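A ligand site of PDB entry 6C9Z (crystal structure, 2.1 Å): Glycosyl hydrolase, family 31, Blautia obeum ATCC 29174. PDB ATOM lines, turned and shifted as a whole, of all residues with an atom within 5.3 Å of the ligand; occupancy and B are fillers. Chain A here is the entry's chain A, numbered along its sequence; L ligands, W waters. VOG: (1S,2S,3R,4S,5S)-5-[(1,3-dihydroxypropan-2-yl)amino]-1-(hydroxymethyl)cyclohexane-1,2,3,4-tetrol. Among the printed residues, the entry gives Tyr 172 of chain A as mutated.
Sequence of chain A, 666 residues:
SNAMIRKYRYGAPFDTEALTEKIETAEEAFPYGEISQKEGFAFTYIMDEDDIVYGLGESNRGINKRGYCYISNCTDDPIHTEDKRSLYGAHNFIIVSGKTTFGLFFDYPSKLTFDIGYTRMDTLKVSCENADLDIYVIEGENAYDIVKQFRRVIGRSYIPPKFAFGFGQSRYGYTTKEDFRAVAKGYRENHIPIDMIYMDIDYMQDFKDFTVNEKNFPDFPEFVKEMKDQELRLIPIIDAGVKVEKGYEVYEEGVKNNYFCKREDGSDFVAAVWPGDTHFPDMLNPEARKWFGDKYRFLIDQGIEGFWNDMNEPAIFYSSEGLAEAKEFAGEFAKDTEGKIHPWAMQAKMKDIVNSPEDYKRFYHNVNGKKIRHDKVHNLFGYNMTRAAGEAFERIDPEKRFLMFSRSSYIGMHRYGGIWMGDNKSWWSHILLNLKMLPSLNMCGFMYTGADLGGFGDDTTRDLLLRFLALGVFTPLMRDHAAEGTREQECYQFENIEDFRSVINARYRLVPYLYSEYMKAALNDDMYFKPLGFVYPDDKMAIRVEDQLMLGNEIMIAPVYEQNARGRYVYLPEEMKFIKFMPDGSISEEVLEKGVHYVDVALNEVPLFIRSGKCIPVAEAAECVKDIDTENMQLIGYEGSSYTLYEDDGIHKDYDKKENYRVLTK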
ATOM      1  N   ASP A  76      14.709  34.960 -10.584  1.00  0.00           N
ATOM      2  CA  ASP A  76      14.354  33.576 -10.872  1.00  0.00           C
ATOM      3  C   ASP A  76      14.477  32.712  -9.604  1.00  0.00           C
ATOM      4  O   ASP A  76      15.556  32.179  -9.318  1.00  0.00           O
ATOM      5  CB  ASP A  76      15.256  33.023 -11.976  1.00  0.00           C
ATOM      6  CG  ASP A  76      14.828  31.631 -12.454  1.00  0.00           C
ATOM      7  OD1 ASP A  76      13.932  31.042 -11.830  1.00  0.00           O
ATOM      8  OD2 ASP A  76      15.386  31.141 -13.453  1.00  0.00           O
ATOM      9  N   PRO A  78      12.649  29.426  -7.725  1.00  0.00           N
ATOM     10  CA  PRO A  78      11.654  28.347  -7.801  1.00  0.00           C
ATOM     11  C   PRO A  78      11.150  27.894  -6.426  1.00  0.00           C
ATOM     12  O   PRO A  78      10.415  26.894  -6.324  1.00  0.00           O
ATOM     13  CB  PRO A  78      12.437  27.220  -8.465  1.00  0.00           C
ATOM     14  CG  PRO A  78      13.847  27.449  -8.010  1.00  0.00           C
ATOM     15  CD  PRO A  78      14.019  28.938  -7.942  1.00  0.00           C
ATOM     16  N   TYR A  88       9.279  37.296  -9.179  1.00  0.00           N
ATOM     17  CA  TYR A  88       9.526  37.608 -10.586  1.00  0.00           C
ATOM     18  C   TYR A  88       9.178  39.045 -10.951  1.00  0.00           C
ATOM     19  O   TYR A  88       9.869  39.662 -11.755  1.00  0.00           O
ATOM     20  CB  TYR A  88       8.744  36.655 -11.486  1.00  0.00           C
ATOM     21  CG  TYR A  88       8.959  35.205 -11.136  1.00  0.00           C
ATOM     22  CD1 TYR A  88      10.092  34.523 -11.576  1.00  0.00           C
ATOM     23  CD2 TYR A  88       8.029  34.519 -10.359  1.00  0.00           C
ATOM     24  CE1 TYR A  88      10.291  33.180 -11.260  1.00  0.00           C
ATOM     25  CE2 TYR A  88       8.224  33.184 -10.038  1.00  0.00           C
ATOM     26  CZ  TYR A  88       9.344  32.526 -10.484  1.00  0.00           C
ATOM     27  OH  TYR A  88       9.523  31.197 -10.165  1.00  0.00           O
ATOM     28  N   TYR A 172       6.659  20.651 -18.696  1.00  0.00           N
ATOM     29  CA  TYR A 172       8.030  20.677 -19.162  1.00  0.00           C
ATOM     30  C   TYR A 172       8.365  19.239 -19.481  1.00  0.00           C
ATOM     31  O   TYR A 172       8.588  18.440 -18.575  1.00  0.00           O
ATOM     32  CB  TYR A 172       8.972  21.281 -18.121  1.00  0.00           C
ATOM     33  CG  TYR A 172      10.448  21.298 -18.501  1.00  0.00           C
ATOM     34  CD1 TYR A 172      10.877  21.008 -19.800  1.00  0.00           C
ATOM     35  CD2 TYR A 172      11.423  21.599 -17.546  1.00  0.00           C
ATOM     36  CE1 TYR A 172      12.239  21.010 -20.144  1.00  0.00           C
ATOM     37  CE2 TYR A 172      12.781  21.612 -17.870  1.00  0.00           C
ATOM     38  CZ  TYR A 172      13.177  21.319 -19.170  1.00  0.00           C
ATOM     39  OH  TYR A 172      14.525  21.334 -19.466  1.00  0.00           O
ATOM     40  N   ASP A 200       6.559  23.639 -24.239  1.00  0.00           N
ATOM     41  CA  ASP A 200       7.731  24.080 -23.501  1.00  0.00           C
ATOM     42  C   ASP A 200       8.982  23.880 -24.345  1.00  0.00           C
ATOM     43  O   ASP A 200       8.924  23.266 -25.421  1.00  0.00           O
ATOM     44  CB  ASP A 200       7.853  23.313 -22.184  1.00  0.00           C
ATOM     45  CG  ASP A 200       8.456  24.150 -21.072  1.00  0.00           C
ATOM     46  OD1 ASP A 200       9.348  24.972 -21.373  1.00  0.00           O
ATOM     47  OD2 ASP A 200       8.028  23.997 -19.906  1.00  0.00           O
ATOM     48  N   ILE A 201      10.101  24.355 -23.843  1.00  0.00           N
ATOM     49  CA  ILE A 201      11.320  24.580 -24.623  1.00  0.00           C
ATOM     50  C   ILE A 201      11.817  23.413 -25.483  1.00  0.00           C
ATOM     51  O   ILE A 201      12.728  23.587 -26.289  1.00  0.00           O
ATOM     52  CB  ILE A 201      12.463  25.060 -23.735  1.00  0.00           C
ATOM     53  CG1 ILE A 201      12.720  24.051 -22.617  1.00  0.00           C
ATOM     54  CG2 ILE A 201      12.119  26.399 -23.131  1.00  0.00           C
ATOM     55  CD1 ILE A 201      13.787  24.486 -21.604  1.00  0.00           C
ATOM     56  N   ILE A 237       6.480  28.556 -26.107  1.00  0.00           N
ATOM     57  CA  ILE A 237       7.258  29.407 -25.233  1.00  0.00           C
ATOM     58  C   ILE A 237       8.375  30.060 -26.039  1.00  0.00           C
ATOM     59  O   ILE A 237       8.866  29.486 -27.021  1.00  0.00           O
ATOM     60  CB  ILE A 237       7.870  28.567 -24.093  1.00  0.00           C
ATOM     61  CG1 ILE A 237       8.391  29.455 -22.960  1.00  0.00           C
ATOM     62  CG2 ILE A 237       8.972  27.637 -24.613  1.00  0.00           C
ATOM     63  CD1 ILE A 237       8.868  28.643 -21.766  1.00  0.00           C
ATOM     64  N   ASP A 239      12.069  32.239 -25.023  1.00  0.00           N
ATOM     65  CA  ASP A 239      12.995  32.607 -23.955  1.00  0.00           C
ATOM     66  C   ASP A 239      13.693  33.930 -24.246  1.00  0.00           C
ATOM     67  O   ASP A 239      13.788  34.353 -25.407  1.00  0.00           O
ATOM     68  CB  ASP A 239      14.036  31.502 -23.757  1.00  0.00           C
ATOM     69  CG  ASP A 239      13.457  30.265 -23.076  1.00  0.00           C
ATOM     70  OD1 ASP A 239      12.425  30.399 -22.362  1.00  0.00           O
ATOM     71  OD2 ASP A 239      14.031  29.170 -23.252  1.00  0.00           O
ATOM     72  N   TRP A 274      19.261  27.600 -21.006  1.00  0.00           N
ATOM     73  CA  TRP A 274      18.967  26.324 -21.689  1.00  0.00           C
ATOM     74  C   TRP A 274      19.832  26.005 -22.910  1.00  0.00           C
ATOM     75  O   TRP A 274      20.270  24.869 -23.065  1.00  0.00           O
ATOM     76  CB  TRP A 274      17.485  26.238 -22.079  1.00  0.00           C
ATOM     77  CG  TRP A 274      16.546  26.586 -20.970  1.00  0.00           C
ATOM     78  CD1 TRP A 274      15.623  27.598 -20.952  1.00  0.00           C
ATOM     79  CD2 TRP A 274      16.429  25.930 -19.694  1.00  0.00           C
ATOM     80  NE1 TRP A 274      14.947  27.610 -19.761  1.00  0.00           N
ATOM     81  CE2 TRP A 274      15.427  26.594 -18.969  1.00  0.00           C
ATOM     82  CE3 TRP A 274      17.089  24.841 -19.105  1.00  0.00           C
ATOM     83  CZ2 TRP A 274      15.048  26.208 -17.680  1.00  0.00           C
ATOM     84  CZ3 TRP A 274      16.716  24.464 -17.824  1.00  0.00           C
ATOM     85  CH2 TRP A 274      15.713  25.146 -17.126  1.00  0.00           C
ATOM     86  N   TRP A 308       3.947  32.327 -24.615  1.00  0.00           N
ATOM     87  CA  TRP A 308       4.412  32.666 -23.278  1.00  0.00           C
ATOM     88  C   TRP A 308       5.908  32.998 -23.231  1.00  0.00           C
ATOM     89  O   TRP A 308       6.734  32.287 -23.805  1.00  0.00           O
ATOM     90  CB  TRP A 308       3.952  31.639 -22.215  1.00  0.00           C
ATOM     91  CG  TRP A 308       4.318  30.168 -22.408  1.00  0.00           C
ATOM     92  CD1 TRP A 308       4.136  29.396 -23.530  1.00  0.00           C
ATOM     93  CD2 TRP A 308       4.869  29.290 -21.407  1.00  0.00           C
ATOM     94  NE1 TRP A 308       4.565  28.099 -23.291  1.00  0.00           N
ATOM     95  CE2 TRP A 308       5.020  28.013 -21.989  1.00  0.00           C
ATOM     96  CE3 TRP A 308       5.247  29.455 -20.067  1.00  0.00           C
ATOM     97  CZ2 TRP A 308       5.529  26.906 -21.291  1.00  0.00           C
ATOM     98  CZ3 TRP A 308       5.770  28.362 -19.379  1.00  0.00           C
ATOM     99  CH2 TRP A 308       5.904  27.110 -19.989  1.00  0.00           C
ATOM    100  N   ASP A 310       9.378  33.658 -21.149  1.00  0.00           N
ATOM    101  CA  ASP A 310       9.976  33.043 -19.949  1.00  0.00           C
ATOM    102  C   ASP A 310      11.464  33.409 -19.786  1.00  0.00           C
ATOM    103  O   ASP A 310      12.094  33.969 -20.703  1.00  0.00           O
ATOM    104  CB  ASP A 310       9.778  31.536 -20.027  1.00  0.00           C
ATOM    105  CG  ASP A 310      10.194  30.791 -18.728  1.00  0.00           C
ATOM    106  OD1 ASP A 310      10.068  31.349 -17.622  1.00  0.00           O
ATOM    107  OD2 ASP A 310      10.653  29.644 -18.851  1.00  0.00           O
ATOM    108  N   MET A 311      12.015  33.107 -18.597  1.00  0.00           N
ATOM    109  CA  MET A 311      13.402  33.422 -18.244  1.00  0.00           C
ATOM    110  C   MET A 311      13.747  34.892 -18.501  1.00  0.00           C
ATOM    111  O   MET A 311      14.904  35.226 -18.727  1.00  0.00           O
ATOM    112  CB  MET A 311      14.386  32.533 -19.017  1.00  0.00           C
ATOM    113  CG  MET A 311      14.025  31.054 -19.079  1.00  0.00           C
ATOM    114  SD  MET A 311      13.947  30.315 -17.433  1.00  0.00           S
ATOM    115  CE  MET A 311      15.694  29.976 -17.078  1.00  0.00           C
ATOM    116  N   ARG A 407       6.638  36.082 -17.491  1.00  0.00           N
ATOM    117  CA  ARG A 407       6.980  35.758 -16.113  1.00  0.00           C
ATOM    118  C   ARG A 407       7.377  37.026 -15.367  1.00  0.00           C
ATOM    119  O   ARG A 407       6.711  37.433 -14.416  1.00  0.00           O
ATOM    120  CB  ARG A 407       8.072  34.684 -16.038  1.00  0.00           C
ATOM    121  CG  ARG A 407       8.239  34.058 -14.630  1.00  0.00           C
ATOM    122  CD  ARG A 407       9.109  32.822 -14.682  1.00  0.00           C
ATOM    123  NE  ARG A 407      10.538  33.163 -14.676  1.00  0.00           N
ATOM    124  CZ  ARG A 407      11.523  32.270 -14.670  1.00  0.00           C
ATOM    125  NH1 ARG A 407      12.787  32.681 -14.671  1.00  0.00           N
ATOM    126  NH2 ARG A 407      11.251  30.977 -14.657  1.00  0.00           N
ATOM    127  N   TRP A 420       1.824  34.804 -15.514  1.00  0.00           N
ATOM    128  CA  TRP A 420       1.532  33.628 -14.722  1.00  0.00           C
ATOM    129  C   TRP A 420       2.467  33.691 -13.529  1.00  0.00           C
ATOM    130  O   TRP A 420       3.543  34.277 -13.629  1.00  0.00           O
ATOM    131  CB  TRP A 420       1.712  32.375 -15.563  1.00  0.00           C
ATOM    132  CG  TRP A 420       3.013  31.659 -15.444  1.00  0.00           C
ATOM    133  CD1 TRP A 420       3.323  30.657 -14.545  1.00  0.00           C
ATOM    134  CD2 TRP A 420       4.167  31.824 -16.277  1.00  0.00           C
ATOM    135  NE1 TRP A 420       4.587  30.215 -14.769  1.00  0.00           N
ATOM    136  CE2 TRP A 420       5.142  30.909 -15.815  1.00  0.00           C
ATOM    137  CE3 TRP A 420       4.479  32.661 -17.358  1.00  0.00           C
ATOM    138  CZ2 TRP A 420       6.400  30.805 -16.398  1.00  0.00           C
ATOM    139  CZ3 TRP A 420       5.737  32.557 -17.941  1.00  0.00           C
ATOM    140  CH2 TRP A 420       6.682  31.639 -17.457  1.00  0.00           C
ATOM    141  N   GLY A 422       4.596  32.009 -12.073  1.00  0.00           N
ATOM    142  CA  GLY A 422       5.913  31.410 -12.054  1.00  0.00           C
ATOM    143  C   GLY A 422       5.952  30.015 -11.454  1.00  0.00           C
ATOM    144  O   GLY A 422       4.943  29.304 -11.467  1.00  0.00           O
ATOM    145  N   ASP A 423       7.109  29.637 -10.904  1.00  0.00           N
ATOM    146  CA  ASP A 423       7.336  28.299 -10.406  1.00  0.00           C
ATOM    147  C   ASP A 423       6.859  28.098  -8.961  1.00  0.00           C
ATOM    148  O   ASP A 423       7.638  28.191  -8.013  1.00  0.00           O
ATOM    149  CB  ASP A 423       8.825  27.928 -10.503  1.00  0.00           C
ATOM    150  CG  ASP A 423       9.339  27.938 -11.930  1.00  0.00           C
ATOM    151  OD1 ASP A 423       8.497  27.842 -12.843  1.00  0.00           O
ATOM    152  OD2 ASP A 423      10.575  28.030 -12.132  1.00  0.00           O
ATOM    153  N   ASP A 452       0.300  27.921 -11.759  1.00  0.00           N
ATOM    154  CA  ASP A 452       0.398  26.535 -12.221  1.00  0.00           C
ATOM    155  C   ASP A 452      -0.469  25.626 -11.345  1.00  0.00           C
ATOM    156  O   ASP A 452      -0.168  25.401 -10.175  1.00  0.00           O
ATOM    157  CB  ASP A 452       1.866  26.065 -12.266  1.00  0.00           C
ATOM    158  CG  ASP A 452       2.673  26.724 -13.389  1.00  0.00           C
ATOM    159  OD1 ASP A 452       2.077  27.443 -14.229  1.00  0.00           O
ATOM    160  OD2 ASP A 452       3.913  26.522 -13.447  1.00  0.00           O
ATOM    161  N   PHE A 456       3.623  23.510  -9.737  1.00  0.00           N
ATOM    162  CA  PHE A 456       4.650  23.251 -10.727  1.00  0.00           C
ATOM    163  C   PHE A 456       5.708  22.278 -10.218  1.00  0.00           C
ATOM    164  O   PHE A 456       5.843  21.168 -10.732  1.00  0.00           O
ATOM    165  CB  PHE A 456       5.299  24.568 -11.192  1.00  0.00           C
ATOM    166  CG  PHE A 456       6.504  24.382 -12.070  1.00  0.00           C
ATOM    167  CD1 PHE A 456       6.356  24.009 -13.404  1.00  0.00           C
ATOM    168  CD2 PHE A 456       7.787  24.600 -11.573  1.00  0.00           C
ATOM    169  CE1 PHE A 456       7.465  23.842 -14.224  1.00  0.00           C
ATOM    170  CE2 PHE A 456       8.908  24.436 -12.372  1.00  0.00           C
ATOM    171  CZ  PHE A 456       8.739  24.058 -13.712  1.00  0.00           C
ATOM    172  N   ARG A 479      -4.461  27.032 -16.169  1.00  0.00           N
ATOM    173  CA  ARG A 479      -3.527  26.132 -16.810  1.00  0.00           C
ATOM    174  C   ARG A 479      -2.907  25.176 -15.781  1.00  0.00           C
ATOM    175  O   ARG A 479      -2.477  25.593 -14.711  1.00  0.00           O
ATOM    176  CB  ARG A 479      -2.426  26.941 -17.495  1.00  0.00           C
ATOM    177  CG  ARG A 479      -1.273  26.077 -17.942  1.00  0.00           C
ATOM    178  CD  ARG A 479      -0.146  26.854 -18.545  1.00  0.00           C
ATOM    179  NE  ARG A 479       0.684  27.544 -17.573  1.00  0.00           N
ATOM    180  CZ  ARG A 479       1.950  27.886 -17.812  1.00  0.00           C
ATOM    181  NH1 ARG A 479       2.509  27.611 -18.987  1.00  0.00           N
ATOM    182  NH2 ARG A 479       2.665  28.509 -16.877  1.00  0.00           N
ATOM    183  N   HIS A 481       0.226  23.022 -15.119  1.00  0.00           N
ATOM    184  CA  HIS A 481       1.628  22.955 -15.561  1.00  0.00           C
ATOM    185  C   HIS A 481       2.472  22.196 -14.528  1.00  0.00           C
ATOM    186  O   HIS A 481       2.221  22.271 -13.325  1.00  0.00           O
ATOM    187  CB  HIS A 481       2.161  24.375 -15.822  1.00  0.00           C
ATOM    188  CG  HIS A 481       3.545  24.417 -16.414  1.00  0.00           C
ATOM    189  ND1 HIS A 481       3.958  23.546 -17.399  1.00  0.00           N
ATOM    190  CD2 HIS A 481       4.594  25.224 -16.154  1.00  0.00           C
ATOM    191  CE1 HIS A 481       5.206  23.822 -17.725  1.00  0.00           C
ATOM    192  NE2 HIS A 481       5.620  24.830 -16.987  1.00  0.00           N
ATOM    193  N   ALA A 482       3.469  21.443 -15.000  1.00  0.00           N
ATOM    194  CA  ALA A 482       4.294  20.609 -14.117  1.00  0.00           C
ATOM    195  C   ALA A 482       5.789  20.655 -14.489  1.00  0.00           C
ATOM    196  O   ALA A 482       6.138  20.803 -15.664  1.00  0.00           O
ATOM    197  CB  ALA A 482       3.785  19.160 -14.118  1.00  0.00           C
HETATM  198  C1  VOG L   1      10.868  25.825 -17.471  1.00  0.00           C
HETATM  199  O1  VOG L   1      11.100  24.855 -16.501  1.00  0.00           O
HETATM  200  C2  VOG L   1       9.394  26.098 -17.525  1.00  0.00           C
HETATM  201  O2  VOG L   1       8.708  24.888 -17.632  1.00  0.00           O
HETATM  202  C3  VOG L   1       8.906  26.832 -16.320  1.00  0.00           C
HETATM  203  O3  VOG L   1       7.553  27.075 -16.472  1.00  0.00           O
HETATM  204  C4  VOG L   1       9.682  28.113 -16.176  1.00  0.00           C
HETATM  205  O4  VOG L   1       9.217  28.847 -15.087  1.00  0.00           O
HETATM  206  C5  VOG L   1      11.146  27.840 -15.998  1.00  0.00           C
HETATM  207  C6  VOG L   1      11.682  27.049 -17.144  1.00  0.00           C
HETATM  208  C7  VOG L   1      11.249  25.300 -18.824  1.00  0.00           C
HETATM  209  O7  VOG L   1      10.966  26.116 -19.889  1.00  0.00           O
HETATM  210  N   VOG L   1      11.365  27.109 -14.760  1.00  0.00           N
HETATM  211  C8  VOG L   1      12.818  27.009 -14.311  1.00  0.00           C
HETATM  212  C9  VOG L   1      13.039  26.100 -13.117  1.00  0.00           C
HETATM  213  O9  VOG L   1      12.496  24.839 -13.222  1.00  0.00           O
HETATM  214  C10 VOG L   1      13.570  28.303 -14.222  1.00  0.00           C
HETATM  215  O10 VOG L   1      13.123  29.168 -13.251  1.00  0.00           O
HETATM  216  O   HOH W   1      11.835  29.994 -10.624  1.00  0.00           O
HETATM  217  O   HOH W   2      12.218  28.270 -20.370  1.00  0.00           O
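An oxygen (O3) of the ligand sits at hydrogen-bond distance from a ring nitrogen (NE2) of His 481 (3.0 Å). The side-chain carboxylate (OD1) of Asp 200 sits at hydrogen-bond distance from an oxygen (O7) of the ligand, at 2.5 Å. The side-chain carboxylate (OD2) of Asp 423 is in salt-bridge range of a nitrogen (N) of the ligand (2.9 Å). The guanidinium group (NH2) of Arg 407 is in hydrogen-bond range of an oxygen (O10) of the ligand, 3.0 Å away. An oxygen (O10) of the ligand sits at hydrogen-bond distance from the side-chain carboxylate (OD1) of Asp 76 (2.5 Å).
The side-chain carboxylate of Asp 76 lies within salt-bridge range of the guanidinium group of Arg 407, 3.3 Å away. The side-chain carboxylate of Asp 423 is in salt-bridge range of the guanidinium group of Arg 407 (3.9 Å). The indole nitrogen (NE1) of Trp 274 sits close to the side-chain sulfur (SD) of Met 311 (3.7 Å). NE1 of Trp 420 sits close to O of Gly 422 (3.4 Å). N of Tyr 172 lies within hydrogen-bond range of O of Ala 482 (3.1 Å). The guanidinium group of Arg 407 is in salt-bridge range of the side-chain carboxylate of Asp 310, 3.2 Å away. N of Asp 423 sits at hydrogen-bond distance from OH of Tyr 88, at 3.0 Å.
Residues that only touch the ligand: Tyr 172 (3.4 Å), Ile 201 (3.5 Å), Ile 237 (3.8 Å), Trp 274 (3.5 Å), Trp 308 (3.6 Å), Asp 310 (3.2 Å), Met 311 (3.8 Å), Trp 420 (3.7 Å) and Phe 456 (3.7 Å). Hydrophobic or aromatic side chains that line the ligand: Tyr 172, Ile 201, Ile 237, Trp 274, Trp 308, Met 311, Trp 420, Phe 456 and His 481. Within 4 Å of the ligand: Asp 76, Tyr 172, Asp 200, Ile 201, Ile 237, Trp 274, Trp 308, Asp 310, Met 311, Arg 407, Trp 420, Asp 423, Phe 456 and His 481. The nearest printed residue that does not touch the ligand is Asp 452 (4.8 Å).
Water W2 lies within hydrogen-bond range of an oxygen (O7) of the ligand (2.5 Å), the side-chain carboxylate (OD2) of Asp 310 (2.6 Å), the indole nitrogen (NE1) of Trp 274 (2.9 Å) and the side-chain carboxylate (OD1) of Asp 239 (2.9 Å). Water W1 lies within hydrogen-bond range of the side-chain carboxylate of Asp 76 (2.6 Å), the side-chain hydroxyl of Tyr 88 (2.6 Å), the side-chain carboxylate of Asp 423 (2.8 Å) and an oxygen (O10) of the ligand (3.0 Å).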
